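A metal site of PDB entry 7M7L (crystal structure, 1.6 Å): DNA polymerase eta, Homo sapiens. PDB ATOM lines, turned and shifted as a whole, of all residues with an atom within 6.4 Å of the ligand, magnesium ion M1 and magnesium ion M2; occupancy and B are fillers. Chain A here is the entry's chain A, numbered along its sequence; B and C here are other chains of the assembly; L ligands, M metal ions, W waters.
Magnesium ion M2 is bound by OD2 of Asp 16 (2.0 Å), OD1 of Asp 118 (2.0 Å), OE2 of Glu 119 (2.1 Å), water W8 (2.1 Å), O3' of DA 8 of chain B (2.2 Å) and O1 of the ligand (2.2 Å).
Residues that only touch magnesium ion M2: Ser 116 (3.7 Å). Five residues have an atom within 4 Å of magnesium ion M2: Asp 16, Ser 116, Asp 118, Glu 119 and DA 8 of chain B. Along chain A the residues within 4 Å of magnesium ion M2 span positions 16 to 119. The nearest printed residue that does not touch magnesium ion M2 is Met 17 (5.4 Å).
Magnesium ion M1 is bound by OD1 of Asp 16, OD2 of Asp 118, O of Met 17, O3 of the ligand, O2 of the ligand and O1 of the ligand. Magnesium ion M1 has six donor atoms within binding distance.
An oxygen (O6) of the ligand sits at hydrogen-bond distance from the side-chain hydroxyl (OH) of Tyr 55 (2.6 Å). A nitrogen (N3) of the ligand is in hydrogen-bond range of O4 of DT 4 of chain C, at 3.1 Å. N of Cys 19 lies within hydrogen-bond range of O6 of the ligand, 2.9 Å away. NH1 of Arg 58 lies within salt-bridge range of O9 of the ligand (3.2 Å). N of Phe 20 lies within hydrogen-bond range of O5 of the ligand, at 3.2 Å. The side-chain amino group of Lys 234 is in salt-bridge range of an oxygen (O6) of the ligand. The backbone NH (N) of Phe 21 lies within hydrogen-bond range of an oxygen (O7) of the ligand (3.1 Å). O4 of the ligand is in salt-bridge range of NH1 of Arg 64.
O of Asp 16 sits at hydrogen-bond distance from NZ of Lys 234 (3.1 Å). The backbone carbonyl oxygen of Ser 216 is in hydrogen-bond range of the backbone NH of Asp 16. N of Asp 118 is in hydrogen-bond range of OG of Ser 116 (3.0 Å). N of Glu 119 sits close to OG of Ser 116, at 3.2 Å. O3' of DA 8 of chain B sits close to the side-chain hydroxyl (OG) of Ser 116 (3.4 Å). OH of Tyr 55 lies within hydrogen-bond range of NH1 of Arg 58, 3.3 Å away. NE of Arg 58 sits at hydrogen-bond distance from O of Val 53 (2.9 Å). NZ of Lys 234 is in salt-bridge range of OD1 of Asp 18 (2.8 Å).
Residues that only touch magnesium ion M1: Lys 234. Of the 26 residues printed, 4 come within 4 Å of magnesium ion M1. The nearest printed residue that does not touch magnesium ion M1 is Asp 18 (4.3 Å).
Merely in contact with the ligand: Asp 18, Ile 51, Ala 52, DT 5 of chain C and Ile 117. Within 4 Å of the ligand: Asp 16, Met 17, Asp 18, Cys 19, Phe 20, Phe 21, Ile 51, Ala 52, Tyr 55, Arg 58, Arg 64, Ile 117, Asp 118, Lys 234, DA 8 of chain B, DT 4 of chain C and DT 5 of chain C. The nearest printed residue that does not touch the ligand is Glu 119 (4.3 Å).
Water W7 lies within hydrogen-bond range of O5 of the ligand (2.7 Å), N of Val 53 (2.8 Å) and NH2 of Arg 58 (2.9 Å). Water W4 lies within hydrogen-bond range of N3 of the ligand (3.1 Å), NE of Arg 64 (3.2 Å) and N7 of DA 8 of chain B (3.4 Å). Water W6 lies within hydrogen-bond range of NH1 of Arg 64, O of Ile 51 and N6 of the ligand. Water W2 bridges N3 of DA 8 of chain B and O10 of the ligand.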
ATOM      1  N   ASP A  16     -22.529 -10.090  11.072  1.00  0.00           N
ATOM      2  CA  ASP A  16     -21.922  -9.981  12.398  1.00  0.00           C
ATOM      3  C   ASP A  16     -20.647  -9.155  12.335  1.00  0.00           C
ATOM      4  O   ASP A  16     -19.723  -9.468  11.572  1.00  0.00           O
ATOM      5  CB  ASP A  16     -21.605 -11.368  12.978  1.00  0.00           C
ATOM      6  CG  ASP A  16     -21.068 -11.294  14.385  1.00  0.00           C
ATOM      7  OD1 ASP A  16     -19.879 -10.979  14.540  1.00  0.00           O
ATOM      8  OD2 ASP A  16     -21.840 -11.497  15.327  1.00  0.00           O
ATOM      9  N   MET A  17     -20.571  -8.142  13.189  1.00  0.00           N
ATOM     10  CA  MET A  17     -19.416  -7.244  13.177  1.00  0.00           C
ATOM     11  C   MET A  17     -18.140  -7.977  13.610  1.00  0.00           C
ATOM     12  O   MET A  17     -18.160  -8.844  14.475  1.00  0.00           O
ATOM     13  CB  MET A  17     -19.684  -6.055  14.106  1.00  0.00           C
ATOM     14  CG  MET A  17     -20.956  -5.280  13.786  1.00  0.00           C
ATOM     15  SD  MET A  17     -21.154  -4.757  12.064  1.00  0.00           S
ATOM     16  CE  MET A  17     -19.814  -3.655  11.860  1.00  0.00           C
ATOM     17  N   ASP A  18     -17.022  -7.627  12.962  1.00  0.00           N
ATOM     18  CA  ASP A  18     -15.728  -8.198  13.355  1.00  0.00           C
ATOM     19  C   ASP A  18     -15.220  -7.472  14.590  1.00  0.00           C
ATOM     20  O   ASP A  18     -15.307  -6.248  14.684  1.00  0.00           O
ATOM     21  CB  ASP A  18     -14.731  -8.073  12.208  1.00  0.00           C
ATOM     22  CG  ASP A  18     -15.174  -8.819  10.935  1.00  0.00           C
ATOM     23  OD1 ASP A  18     -15.932  -9.812  11.032  1.00  0.00           O
ATOM     24  OD2 ASP A  18     -14.746  -8.428   9.850  1.00  0.00           O
ATOM     25  N   CYS A  19     -14.721  -8.257  15.554  1.00  0.00           N
ATOM     26  CA  CYS A  19     -14.214  -7.780  16.852  1.00  0.00           C
ATOM     27  C   CYS A  19     -14.843  -6.454  17.239  1.00  0.00           C
ATOM     28  O   CYS A  19     -14.165  -5.419  17.333  1.00  0.00           O
ATOM     29  CB  CYS A  19     -12.674  -7.715  16.853  1.00  0.00           C
ATOM     30  SG  CYS A  19     -11.849  -6.782  15.535  1.00  0.00           S
ATOM     31  N   PHE A  20     -16.157  -6.464  17.454  1.00  0.00           N
ATOM     32  CA  PHE A  20     -16.940  -5.226  17.378  1.00  0.00           C
ATOM     33  C   PHE A  20     -16.453  -4.137  18.326  1.00  0.00           C
ATOM     34  O   PHE A  20     -16.197  -3.006  17.897  1.00  0.00           O
ATOM     35  CB  PHE A  20     -18.407  -5.520  17.610  1.00  0.00           C
ATOM     36  CG  PHE A  20     -19.284  -4.327  17.459  1.00  0.00           C
ATOM     37  CD1 PHE A  20     -19.116  -3.445  16.399  1.00  0.00           C
ATOM     38  CD2 PHE A  20     -20.290  -4.090  18.371  1.00  0.00           C
ATOM     39  CE1 PHE A  20     -19.946  -2.334  16.245  1.00  0.00           C
ATOM     40  CE2 PHE A  20     -21.128  -2.970  18.224  1.00  0.00           C
ATOM     41  CZ  PHE A  20     -20.948  -2.109  17.162  1.00  0.00           C
ATOM     42  N   PHE A  21     -16.394  -4.421  19.641  1.00  0.00           N
ATOM     43  CA  PHE A  21     -16.044  -3.349  20.580  1.00  0.00           C
ATOM     44  C   PHE A  21     -14.642  -2.817  20.302  1.00  0.00           C
ATOM     45  O   PHE A  21     -14.377  -1.626  20.471  1.00  0.00           O
ATOM     46  CB  PHE A  21     -16.133  -3.809  22.032  1.00  0.00           C
ATOM     47  CG  PHE A  21     -17.546  -4.061  22.547  1.00  0.00           C
ATOM     48  CD1 PHE A  21     -18.640  -4.141  21.699  1.00  0.00           C
ATOM     49  CD2 PHE A  21     -17.751  -4.223  23.900  1.00  0.00           C
ATOM     50  CE1 PHE A  21     -19.917  -4.384  22.204  1.00  0.00           C
ATOM     51  CE2 PHE A  21     -19.027  -4.462  24.416  1.00  0.00           C
ATOM     52  CZ  PHE A  21     -20.108  -4.539  23.566  1.00  0.00           C
ATOM     53  N   VAL A  22     -13.735  -3.696  19.852  1.00  0.00           N
ATOM     54  CA  VAL A  22     -12.404  -3.242  19.456  1.00  0.00           C
ATOM     55  C   VAL A  22     -12.498  -2.259  18.294  1.00  0.00           C
ATOM     56  O   VAL A  22     -11.839  -1.226  18.293  1.00  0.00           O
ATOM     57  CB  VAL A  22     -11.500  -4.442  19.107  1.00  0.00           C
ATOM     58  CG1 VAL A  22     -10.237  -3.968  18.374  1.00  0.00           C
ATOM     59  CG2 VAL A  22     -11.128  -5.215  20.360  1.00  0.00           C
ATOM     60  N   GLN A  41     -12.942  -4.593  30.771  1.00  0.00           N
ATOM     61  CA  GLN A  41     -13.858  -4.041  31.795  1.00  0.00           C
ATOM     62  C   GLN A  41     -13.202  -4.159  33.164  1.00  0.00           C
ATOM     63  O   GLN A  41     -12.789  -5.226  33.511  1.00  0.00           O
ATOM     64  CB  GLN A  41     -15.216  -4.745  31.934  1.00  0.00           C
ATOM     65  CG  GLN A  41     -15.979  -5.009  30.661  1.00  0.00           C
ATOM     66  CD  GLN A  41     -17.330  -5.543  31.045  1.00  0.00           C
ATOM     67  OE1 GLN A  41     -18.339  -4.865  30.901  1.00  0.00           O
ATOM     68  NE2 GLN A  41     -17.349  -6.757  31.582  1.00  0.00           N
ATOM     69  N   ILE A  51     -13.235  -8.431  27.060  1.00  0.00           N
ATOM     70  CA  ILE A  51     -14.506  -8.771  26.436  1.00  0.00           C
ATOM     71  C   ILE A  51     -14.470  -8.734  24.911  1.00  0.00           C
ATOM     72  O   ILE A  51     -15.425  -9.216  24.285  1.00  0.00           O
ATOM     73  CB  ILE A  51     -15.668  -7.885  26.968  1.00  0.00           C
ATOM     74  CG1 ILE A  51     -15.396  -6.400  26.725  1.00  0.00           C
ATOM     75  CG2 ILE A  51     -15.890  -8.159  28.451  1.00  0.00           C
ATOM     76  CD1 ILE A  51     -16.631  -5.525  27.050  1.00  0.00           C
ATOM     77  N   ALA A  52     -13.400  -8.218  24.287  1.00  0.00           N
ATOM     78  CA  ALA A  52     -13.284  -8.203  22.832  1.00  0.00           C
ATOM     79  C   ALA A  52     -11.805  -8.136  22.461  1.00  0.00           C
ATOM     80  O   ALA A  52     -11.017  -7.511  23.177  1.00  0.00           O
ATOM     81  CB  ALA A  52     -14.030  -7.011  22.205  1.00  0.00           C
ATOM     82  N   VAL A  53     -11.431  -8.787  21.355  1.00  0.00           N
ATOM     83  CA  VAL A  53     -10.026  -9.023  21.016  1.00  0.00           C
ATOM     84  C   VAL A  53      -9.819  -8.821  19.518  1.00  0.00           C
ATOM     85  O   VAL A  53     -10.506  -9.462  18.707  1.00  0.00           O
ATOM     86  CB  VAL A  53      -9.585 -10.459  21.395  1.00  0.00           C
ATOM     87  CG1 VAL A  53      -8.082 -10.615  21.225  1.00  0.00           C
ATOM     88  CG2 VAL A  53      -9.975 -10.802  22.814  1.00  0.00           C
ATOM     89  N   TYR A  55      -8.014  -9.240  15.828  1.00  0.00           N
ATOM     90  CA  TYR A  55      -7.515 -10.474  15.218  1.00  0.00           C
ATOM     91  C   TYR A  55      -5.992 -10.582  15.351  1.00  0.00           C
ATOM     92  O   TYR A  55      -5.453 -11.679  15.543  1.00  0.00           O
ATOM     93  CB  TYR A  55      -7.978 -10.576  13.766  1.00  0.00           C
ATOM     94  CG  TYR A  55      -9.409 -11.062  13.706  1.00  0.00           C
ATOM     95  CD1 TYR A  55     -10.475 -10.172  13.902  1.00  0.00           C
ATOM     96  CD2 TYR A  55      -9.705 -12.407  13.544  1.00  0.00           C
ATOM     97  CE1 TYR A  55     -11.791 -10.621  13.898  1.00  0.00           C
ATOM     98  CE2 TYR A  55     -11.013 -12.864  13.533  1.00  0.00           C
ATOM     99  CZ  TYR A  55     -12.051 -11.972  13.716  1.00  0.00           C
ATOM    100  OH  TYR A  55     -13.344 -12.423  13.712  1.00  0.00           O
ATOM    101  N   ARG A  58      -5.616 -12.040  18.705  1.00  0.00           N
ATOM    102  CA  ARG A  58      -6.005 -13.449  18.732  1.00  0.00           C
ATOM    103  C   ARG A  58      -4.879 -14.344  18.247  1.00  0.00           C
ATOM    104  O   ARG A  58      -4.750 -15.484  18.707  1.00  0.00           O
ATOM    105  CB  ARG A  58      -7.251 -13.676  17.871  1.00  0.00           C
ATOM    106  CG  ARG A  58      -8.450 -12.914  18.345  1.00  0.00           C
ATOM    107  CD  ARG A  58      -9.656 -13.210  17.498  1.00  0.00           C
ATOM    108  NE  ARG A  58     -10.670 -12.193  17.750  1.00  0.00           N
ATOM    109  CZ  ARG A  58     -11.940 -12.268  17.378  1.00  0.00           C
ATOM    110  NH1 ARG A  58     -12.379 -13.344  16.723  1.00  0.00           N
ATOM    111  NH2 ARG A  58     -12.766 -11.260  17.658  1.00  0.00           N
ATOM    112  N   ARG A  64     -11.460 -13.645  24.723  1.00  0.00           N
ATOM    113  CA  ARG A  64     -12.480 -13.148  25.634  1.00  0.00           C
ATOM    114  C   ARG A  64     -12.466 -13.965  26.928  1.00  0.00           C
ATOM    115  O   ARG A  64     -12.160 -15.163  26.933  1.00  0.00           O
ATOM    116  CB  ARG A  64     -13.849 -13.251  24.944  1.00  0.00           C
ATOM    117  CG  ARG A  64     -15.061 -12.836  25.754  1.00  0.00           C
ATOM    118  CD  ARG A  64     -16.303 -12.962  24.865  1.00  0.00           C
ATOM    119  NE  ARG A  64     -16.296 -14.236  24.150  1.00  0.00           N
ATOM    120  CZ  ARG A  64     -16.824 -14.437  22.941  1.00  0.00           C
ATOM    121  NH1 ARG A  64     -17.412 -13.448  22.277  1.00  0.00           N
ATOM    122  NH2 ARG A  64     -16.748 -15.642  22.379  1.00  0.00           N
ATOM    123  N   LEU A  92     -22.140   0.464  28.819  1.00  0.00           N
ATOM    124  CA  LEU A  92     -21.955  -0.008  27.450  1.00  0.00           C
ATOM    125  C   LEU A  92     -22.564   0.929  26.410  1.00  0.00           C
ATOM    126  O   LEU A  92     -22.703   0.542  25.235  1.00  0.00           O
ATOM    127  CB  LEU A  92     -22.539  -1.418  27.323  1.00  0.00           C
ATOM    128  CG  LEU A  92     -21.968  -2.435  28.319  1.00  0.00           C
ATOM    129  CD1 LEU A  92     -22.667  -3.772  28.159  1.00  0.00           C
ATOM    130  CD2 LEU A  92     -20.483  -2.578  28.091  1.00  0.00           C
ATOM    131  N   SER A 116     -28.122  -9.525  18.321  1.00  0.00           N
ATOM    132  CA  SER A 116     -27.226  -9.201  19.426  1.00  0.00           C
ATOM    133  C   SER A 116     -26.829  -7.740  19.262  1.00  0.00           C
ATOM    134  O   SER A 116     -27.256  -7.065  18.326  1.00  0.00           O
ATOM    135  CB  SER A 116     -25.995 -10.117  19.459  1.00  0.00           C
ATOM    136  OG  SER A 116     -25.036  -9.719  18.489  1.00  0.00           O
ATOM    137  N   ILE A 117     -25.954  -7.275  20.154  1.00  0.00           N
ATOM    138  CA  ILE A 117     -25.454  -5.920  19.984  1.00  0.00           C
ATOM    139  C   ILE A 117     -24.697  -5.761  18.663  1.00  0.00           C
ATOM    140  O   ILE A 117     -24.592  -4.661  18.134  1.00  0.00           O
ATOM    141  CB  ILE A 117     -24.572  -5.510  21.185  1.00  0.00           C
ATOM    142  CG1 ILE A 117     -24.459  -3.981  21.264  1.00  0.00           C
ATOM    143  CG2 ILE A 117     -23.207  -6.151  21.087  1.00  0.00           C
ATOM    144  CD1 ILE A 117     -23.825  -3.483  22.570  1.00  0.00           C
ATOM    145  N   ASP A 118     -24.171  -6.856  18.095  1.00  0.00           N
ATOM    146  CA  ASP A 118     -23.324  -6.696  16.920  1.00  0.00           C
ATOM    147  C   ASP A 118     -23.779  -7.539  15.728  1.00  0.00           C
ATOM    148  O   ASP A 118     -23.000  -7.702  14.764  1.00  0.00           O
ATOM    149  CB  ASP A 118     -21.855  -6.983  17.240  1.00  0.00           C
ATOM    150  CG  ASP A 118     -21.446  -8.430  16.982  1.00  0.00           C
ATOM    151  OD1 ASP A 118     -22.194  -9.378  17.361  1.00  0.00           O
ATOM    152  OD2 ASP A 118     -20.356  -8.602  16.395  1.00  0.00           O
ATOM    153  N   GLU A 119     -24.997  -8.063  15.728  1.00  0.00           N
ATOM    154  CA  GLU A 119     -25.416  -8.850  14.577  1.00  0.00           C
ATOM    155  C   GLU A 119     -26.917  -8.809  14.373  1.00  0.00           C
ATOM    156  O   GLU A 119     -27.701  -8.658  15.331  1.00  0.00           O
ATOM    157  CB  GLU A 119     -24.974 -10.311  14.676  1.00  0.00           C
ATOM    158  CG  GLU A 119     -25.707 -11.126  15.721  1.00  0.00           C
ATOM    159  CD  GLU A 119     -24.795 -12.158  16.324  1.00  0.00           C
ATOM    160  OE1 GLU A 119     -24.891 -13.343  15.943  1.00  0.00           O
ATOM    161  OE2 GLU A 119     -23.955 -11.790  17.169  1.00  0.00           O
ATOM    162  N   SER A 216     -18.522  -9.511   8.876  1.00  0.00           N
ATOM    163  CA  SER A 216     -18.653 -10.706   8.073  1.00  0.00           C
ATOM    164  C   SER A 216     -20.127 -11.048   7.928  1.00  0.00           C
ATOM    165  O   SER A 216     -20.981 -10.474   8.610  1.00  0.00           O
ATOM    166  CB  SER A 216     -17.883 -11.879   8.692  1.00  0.00           C
ATOM    167  OG  SER A 216     -16.496 -11.550   8.760  1.00  0.00           O
ATOM    168  N   LYS A 234     -14.655 -15.466   8.710  1.00  0.00           N
ATOM    169  CA  LYS A 234     -14.291 -14.269   9.451  1.00  0.00           C
ATOM    170  C   LYS A 234     -12.773 -14.099   9.520  1.00  0.00           C
ATOM    171  O   LYS A 234     -12.050 -15.094   9.667  1.00  0.00           O
ATOM    172  CB  LYS A 234     -14.851 -14.339  10.870  1.00  0.00           C
ATOM    173  CG  LYS A 234     -16.070 -13.522  11.109  1.00  0.00           C
ATOM    174  CD  LYS A 234     -16.522 -13.577  12.550  1.00  0.00           C
ATOM    175  CE  LYS A 234     -17.785 -12.750  12.745  1.00  0.00           C
ATOM    176  NZ  LYS A 234     -17.525 -11.277  12.796  1.00  0.00           N
ATOM    177  N   PRO A 235     -12.259 -12.867   9.471  1.00  0.00           N
ATOM    178  CA  PRO A 235     -13.004 -11.603   9.394  1.00  0.00           C
ATOM    179  C   PRO A 235     -13.089 -11.029   7.980  1.00  0.00           C
ATOM    180  O   PRO A 235     -12.375 -11.485   7.088  1.00  0.00           O
ATOM    181  CB  PRO A 235     -12.198 -10.669  10.282  1.00  0.00           C
ATOM    182  CG  PRO A 235     -10.770 -11.112   9.999  1.00  0.00           C
ATOM    183  CD  PRO A 235     -10.832 -12.610   9.736  1.00  0.00           C
ATOM    184  P    DA B   8     -23.314 -16.902  20.415  1.00  0.00           P
ATOM    185  OP1  DA B   8     -22.938 -17.055  18.991  1.00  0.00           O
ATOM    186  OP2  DA B   8     -22.272 -17.144  21.440  1.00  0.00           O
ATOM    187  O5'  DA B   8     -24.075 -15.476  20.683  1.00  0.00           O
ATOM    188  C5'  DA B   8     -24.387 -14.438  19.680  1.00  0.00           C
ATOM    189  C4'  DA B   8     -23.952 -13.128  20.321  1.00  0.00           C
ATOM    190  O4'  DA B   8     -24.202 -13.142  21.749  1.00  0.00           O
ATOM    191  C3'  DA B   8     -22.477 -12.804  20.141  1.00  0.00           C
ATOM    192  O3'  DA B   8     -22.325 -11.548  19.454  1.00  0.00           O
ATOM    193  C2'  DA B   8     -21.890 -12.781  21.565  1.00  0.00           C
ATOM    194  C1'  DA B   8     -23.117 -12.556  22.437  1.00  0.00           C
ATOM    195  N9   DA B   8     -23.008 -13.200  23.748  1.00  0.00           N
ATOM    196  C8   DA B   8     -22.837 -14.537  24.004  1.00  0.00           C
ATOM    197  N7   DA B   8     -22.780 -14.835  25.282  1.00  0.00           N
ATOM    198  C5   DA B   8     -22.926 -13.607  25.912  1.00  0.00           C
ATOM    199  C6   DA B   8     -22.939 -13.226  27.267  1.00  0.00           C
ATOM    200  N6   DA B   8     -22.823 -14.096  28.278  1.00  0.00           N
ATOM    201  N1   DA B   8     -23.099 -11.928  27.550  1.00  0.00           N
ATOM    202  C2   DA B   8     -23.215 -11.058  26.539  1.00  0.00           C
ATOM    203  N3   DA B   8     -23.221 -11.292  25.237  1.00  0.00           N
ATOM    204  C4   DA B   8     -23.065 -12.591  24.975  1.00  0.00           C
ATOM    205  P    DT C   3     -13.247 -16.432  37.671  1.00  0.00           P
ATOM    206  OP1  DT C   3     -13.869 -17.569  38.373  1.00  0.00           O
ATOM    207  OP2  DT C   3     -11.907 -16.562  37.058  1.00  0.00           O
ATOM    208  O5'  DT C   3     -14.239 -15.937  36.514  1.00  0.00           O
ATOM    209  C5'  DT C   3     -13.726 -15.224  35.399  1.00  0.00           C
ATOM    210  C4'  DT C   3     -14.675 -14.121  34.974  1.00  0.00           C
ATOM    211  O4'  DT C   3     -14.990 -14.275  33.567  1.00  0.00           O
ATOM    212  C3'  DT C   3     -16.027 -14.147  35.678  1.00  0.00           C
ATOM    213  O3'  DT C   3     -16.609 -12.867  35.653  1.00  0.00           O
ATOM    214  C2'  DT C   3     -16.819 -15.129  34.819  1.00  0.00           C
ATOM    215  C1'  DT C   3     -16.266 -14.883  33.420  1.00  0.00           C
ATOM    216  N1   DT C   3     -16.097 -16.138  32.637  1.00  0.00           N
ATOM    217  C2   DT C   3     -16.435 -16.146  31.305  1.00  0.00           C
ATOM    218  O2   DT C   3     -16.871 -15.175  30.717  1.00  0.00           O
ATOM    219  N3   DT C   3     -16.248 -17.361  30.678  1.00  0.00           N
ATOM    220  C4   DT C   3     -15.756 -18.525  31.252  1.00  0.00           C
ATOM    221  O4   DT C   3     -15.626 -19.562  30.602  1.00  0.00           O
ATOM    222  C5   DT C   3     -15.420 -18.439  32.651  1.00  0.00           C
ATOM    223  C7   DT C   3     -14.893 -19.638  33.376  1.00  0.00           C
ATOM    224  C6   DT C   3     -15.606 -17.264  33.271  1.00  0.00           C
ATOM    225  P    DT C   4     -17.351 -12.291  36.951  1.00  0.00           P
ATOM    226  OP1  DT C   4     -16.352 -12.089  38.013  1.00  0.00           O
ATOM    227  OP2  DT C   4     -18.553 -13.124  37.175  1.00  0.00           O
ATOM    228  O5'  DT C   4     -17.875 -10.868  36.473  1.00  0.00           O
ATOM    229  C5'  DT C   4     -16.965  -9.908  36.008  1.00  0.00           C
ATOM    230  C4'  DT C   4     -17.697  -8.912  35.134  1.00  0.00           C
ATOM    231  O4'  DT C   4     -17.837  -9.450  33.802  1.00  0.00           O
ATOM    232  C3'  DT C   4     -19.100  -8.551  35.597  1.00  0.00           C
ATOM    233  O3'  DT C   4     -19.281  -7.179  35.382  1.00  0.00           O
ATOM    234  C2'  DT C   4     -19.997  -9.394  34.667  1.00  0.00           C
ATOM    235  C1'  DT C   4     -19.180  -9.381  33.389  1.00  0.00           C
ATOM    236  N1   DT C   4     -19.429 -10.529  32.486  1.00  0.00           N
ATOM    237  C2   DT C   4     -19.521 -10.270  31.150  1.00  0.00           C
ATOM    238  O2   DT C   4     -19.442  -9.152  30.689  1.00  0.00           O
ATOM    239  N3   DT C   4     -19.721 -11.375  30.368  1.00  0.00           N
ATOM    240  C4   DT C   4     -19.816 -12.679  30.781  1.00  0.00           C
ATOM    241  O4   DT C   4     -19.987 -13.596  29.981  1.00  0.00           O
ATOM    242  C5   DT C   4     -19.702 -12.891  32.206  1.00  0.00           C
ATOM    243  C7   DT C   4     -19.794 -14.282  32.781  1.00  0.00           C
ATOM    244  C6   DT C   4     -19.504 -11.810  32.987  1.00  0.00           C
ATOM    245  P    DT C   5     -20.664  -6.466  35.753  1.00  0.00           P
ATOM    246  OP1  DT C   5     -20.315  -5.100  36.205  1.00  0.00           O
ATOM    247  OP2  DT C   5     -21.467  -7.355  36.625  1.00  0.00           O
ATOM    248  O5'  DT C   5     -21.422  -6.391  34.362  1.00  0.00           O
ATOM    249  C5'  DT C   5     -20.958  -5.503  33.354  1.00  0.00           C
ATOM    250  C4'  DT C   5     -21.895  -5.557  32.169  1.00  0.00           C
ATOM    251  O4'  DT C   5     -21.837  -6.869  31.563  1.00  0.00           O
ATOM    252  C3'  DT C   5     -23.362  -5.303  32.514  1.00  0.00           C
ATOM    253  O3'  DT C   5     -23.920  -4.423  31.538  1.00  0.00           O
ATOM    254  C2'  DT C   5     -23.984  -6.704  32.440  1.00  0.00           C
ATOM    255  C1'  DT C   5     -23.149  -7.305  31.319  1.00  0.00           C
ATOM    256  N1   DT C   5     -23.144  -8.767  31.253  1.00  0.00           N
ATOM    257  C2   DT C   5     -23.112  -9.361  30.022  1.00  0.00           C
ATOM    258  O2   DT C   5     -23.095  -8.735  28.991  1.00  0.00           O
ATOM    259  N3   DT C   5     -23.094 -10.730  30.050  1.00  0.00           N
ATOM    260  C4   DT C   5     -23.095 -11.551  31.154  1.00  0.00           C
ATOM    261  O4   DT C   5     -23.088 -12.773  31.061  1.00  0.00           O
ATOM    262  C5   DT C   5     -23.128 -10.864  32.425  1.00  0.00           C
ATOM    263  C7   DT C   5     -23.129 -11.653  33.699  1.00  0.00           C
ATOM    264  C6   DT C   5     -23.144  -9.525  32.420  1.00  0.00           C
HETATM  265  N1  LIG L   1     -19.757 -10.756  27.714  1.00  0.00           N
HETATM  266  C1  LIG L   1     -19.787  -9.453  27.413  1.00  0.00           C
HETATM  267  N2  LIG L   1     -19.722  -8.875  26.216  1.00  0.00           N
HETATM  268  C2  LIG L   1     -19.598  -9.795  25.255  1.00  0.00           C
HETATM  269  C3  LIG L   1     -19.552 -11.157  25.407  1.00  0.00           C
HETATM  270  C4  LIG L   1     -19.637 -11.654  26.713  1.00  0.00           C
HETATM  271  N3  LIG L   1     -19.598 -12.956  26.971  1.00  0.00           N
HETATM  272  N4  LIG L   1     -19.428 -11.775  24.171  1.00  0.00           N
HETATM  273  C5  LIG L   1     -19.398 -10.786  23.312  1.00  0.00           C
HETATM  274  N5  LIG L   1     -19.495  -9.564  23.911  1.00  0.00           N
HETATM  275  P1  LIG L   1     -19.060 -11.319  19.123  1.00  0.00           P
HETATM  276  P2  LIG L   1     -16.674  -9.988  18.225  1.00  0.00           P
HETATM  277  P3  LIG L   1     -15.956 -11.651  16.003  1.00  0.00           P
HETATM  278  C6  LIG L   1     -19.490  -8.245  23.270  1.00  0.00           C
HETATM  279  O1  LIG L   1     -19.775 -11.165  17.872  1.00  0.00           O
HETATM  280  O2  LIG L   1     -17.523  -9.114  17.423  1.00  0.00           O
HETATM  281  O3  LIG L   1     -17.414 -11.569  15.814  1.00  0.00           O
HETATM  282  C7  LIG L   1     -18.102  -7.751  22.879  1.00  0.00           C
HETATM  283  O4  LIG L   1     -19.313 -12.711  19.748  1.00  0.00           O
HETATM  284  O5  LIG L   1     -15.817  -9.158  19.215  1.00  0.00           O
HETATM  285  O6  LIG L   1     -15.196 -11.032  14.893  1.00  0.00           O
HETATM  286  C8  LIG L   1     -18.018  -8.127  21.402  1.00  0.00           C
HETATM  287  O7  LIG L   1     -17.155  -7.271  20.668  1.00  0.00           O
HETATM  288  N6  LIG L   1     -17.462 -11.141  19.026  1.00  0.00           N
HETATM  289  O8  LIG L   1     -15.640 -10.756  17.289  1.00  0.00           O
HETATM  290  O9  LIG L   1     -15.493 -13.041  16.343  1.00  0.00           O
HETATM  291  C9  LIG L   1     -19.459  -7.978  20.941  1.00  0.00           C
HETATM  292  O10 LIG L   1     -20.272  -8.311  22.084  1.00  0.00           O
HETATM  293  C10 LIG L   1     -19.842  -8.884  19.801  1.00  0.00           C
HETATM  294  O11 LIG L   1     -19.642 -10.254  20.175  1.00  0.00           O
HETATM  295 MG    MG M   1     -18.892 -10.028  16.035  1.00  0.00          MG
HETATM  296 MG    MG M   2     -21.899 -11.403  17.327  1.00  0.00          MG
HETATM  297  O   HOH W   1     -18.977 -13.939  15.823  1.00  0.00           O
HETATM  298  O   HOH W   2     -22.849  -8.687  24.168  1.00  0.00           O
HETATM  299  O   HOH W   3     -22.694  -9.584  21.206  1.00  0.00           O
HETATM  300  O   HOH W   4     -19.448 -14.839  24.544  1.00  0.00           O
HETATM  301  O   HOH W   5     -20.689  -6.274  26.700  1.00  0.00           O
HETATM  302  O   HOH W   6     -16.117 -11.099  22.073  1.00  0.00           O
HETATM  303  O   HOH W   7     -13.550 -10.222  20.216  1.00  0.00           O
HETATM  304  O   HOH W   8     -21.294 -13.443  17.341  1.00  0.00           O
HETATM  305  O   HOH W   9     -19.537 -15.311  19.546  1.00  0.00           O
HETATM  306  O   HOH W  10     -15.499 -13.889  18.892  1.00  0.00           O
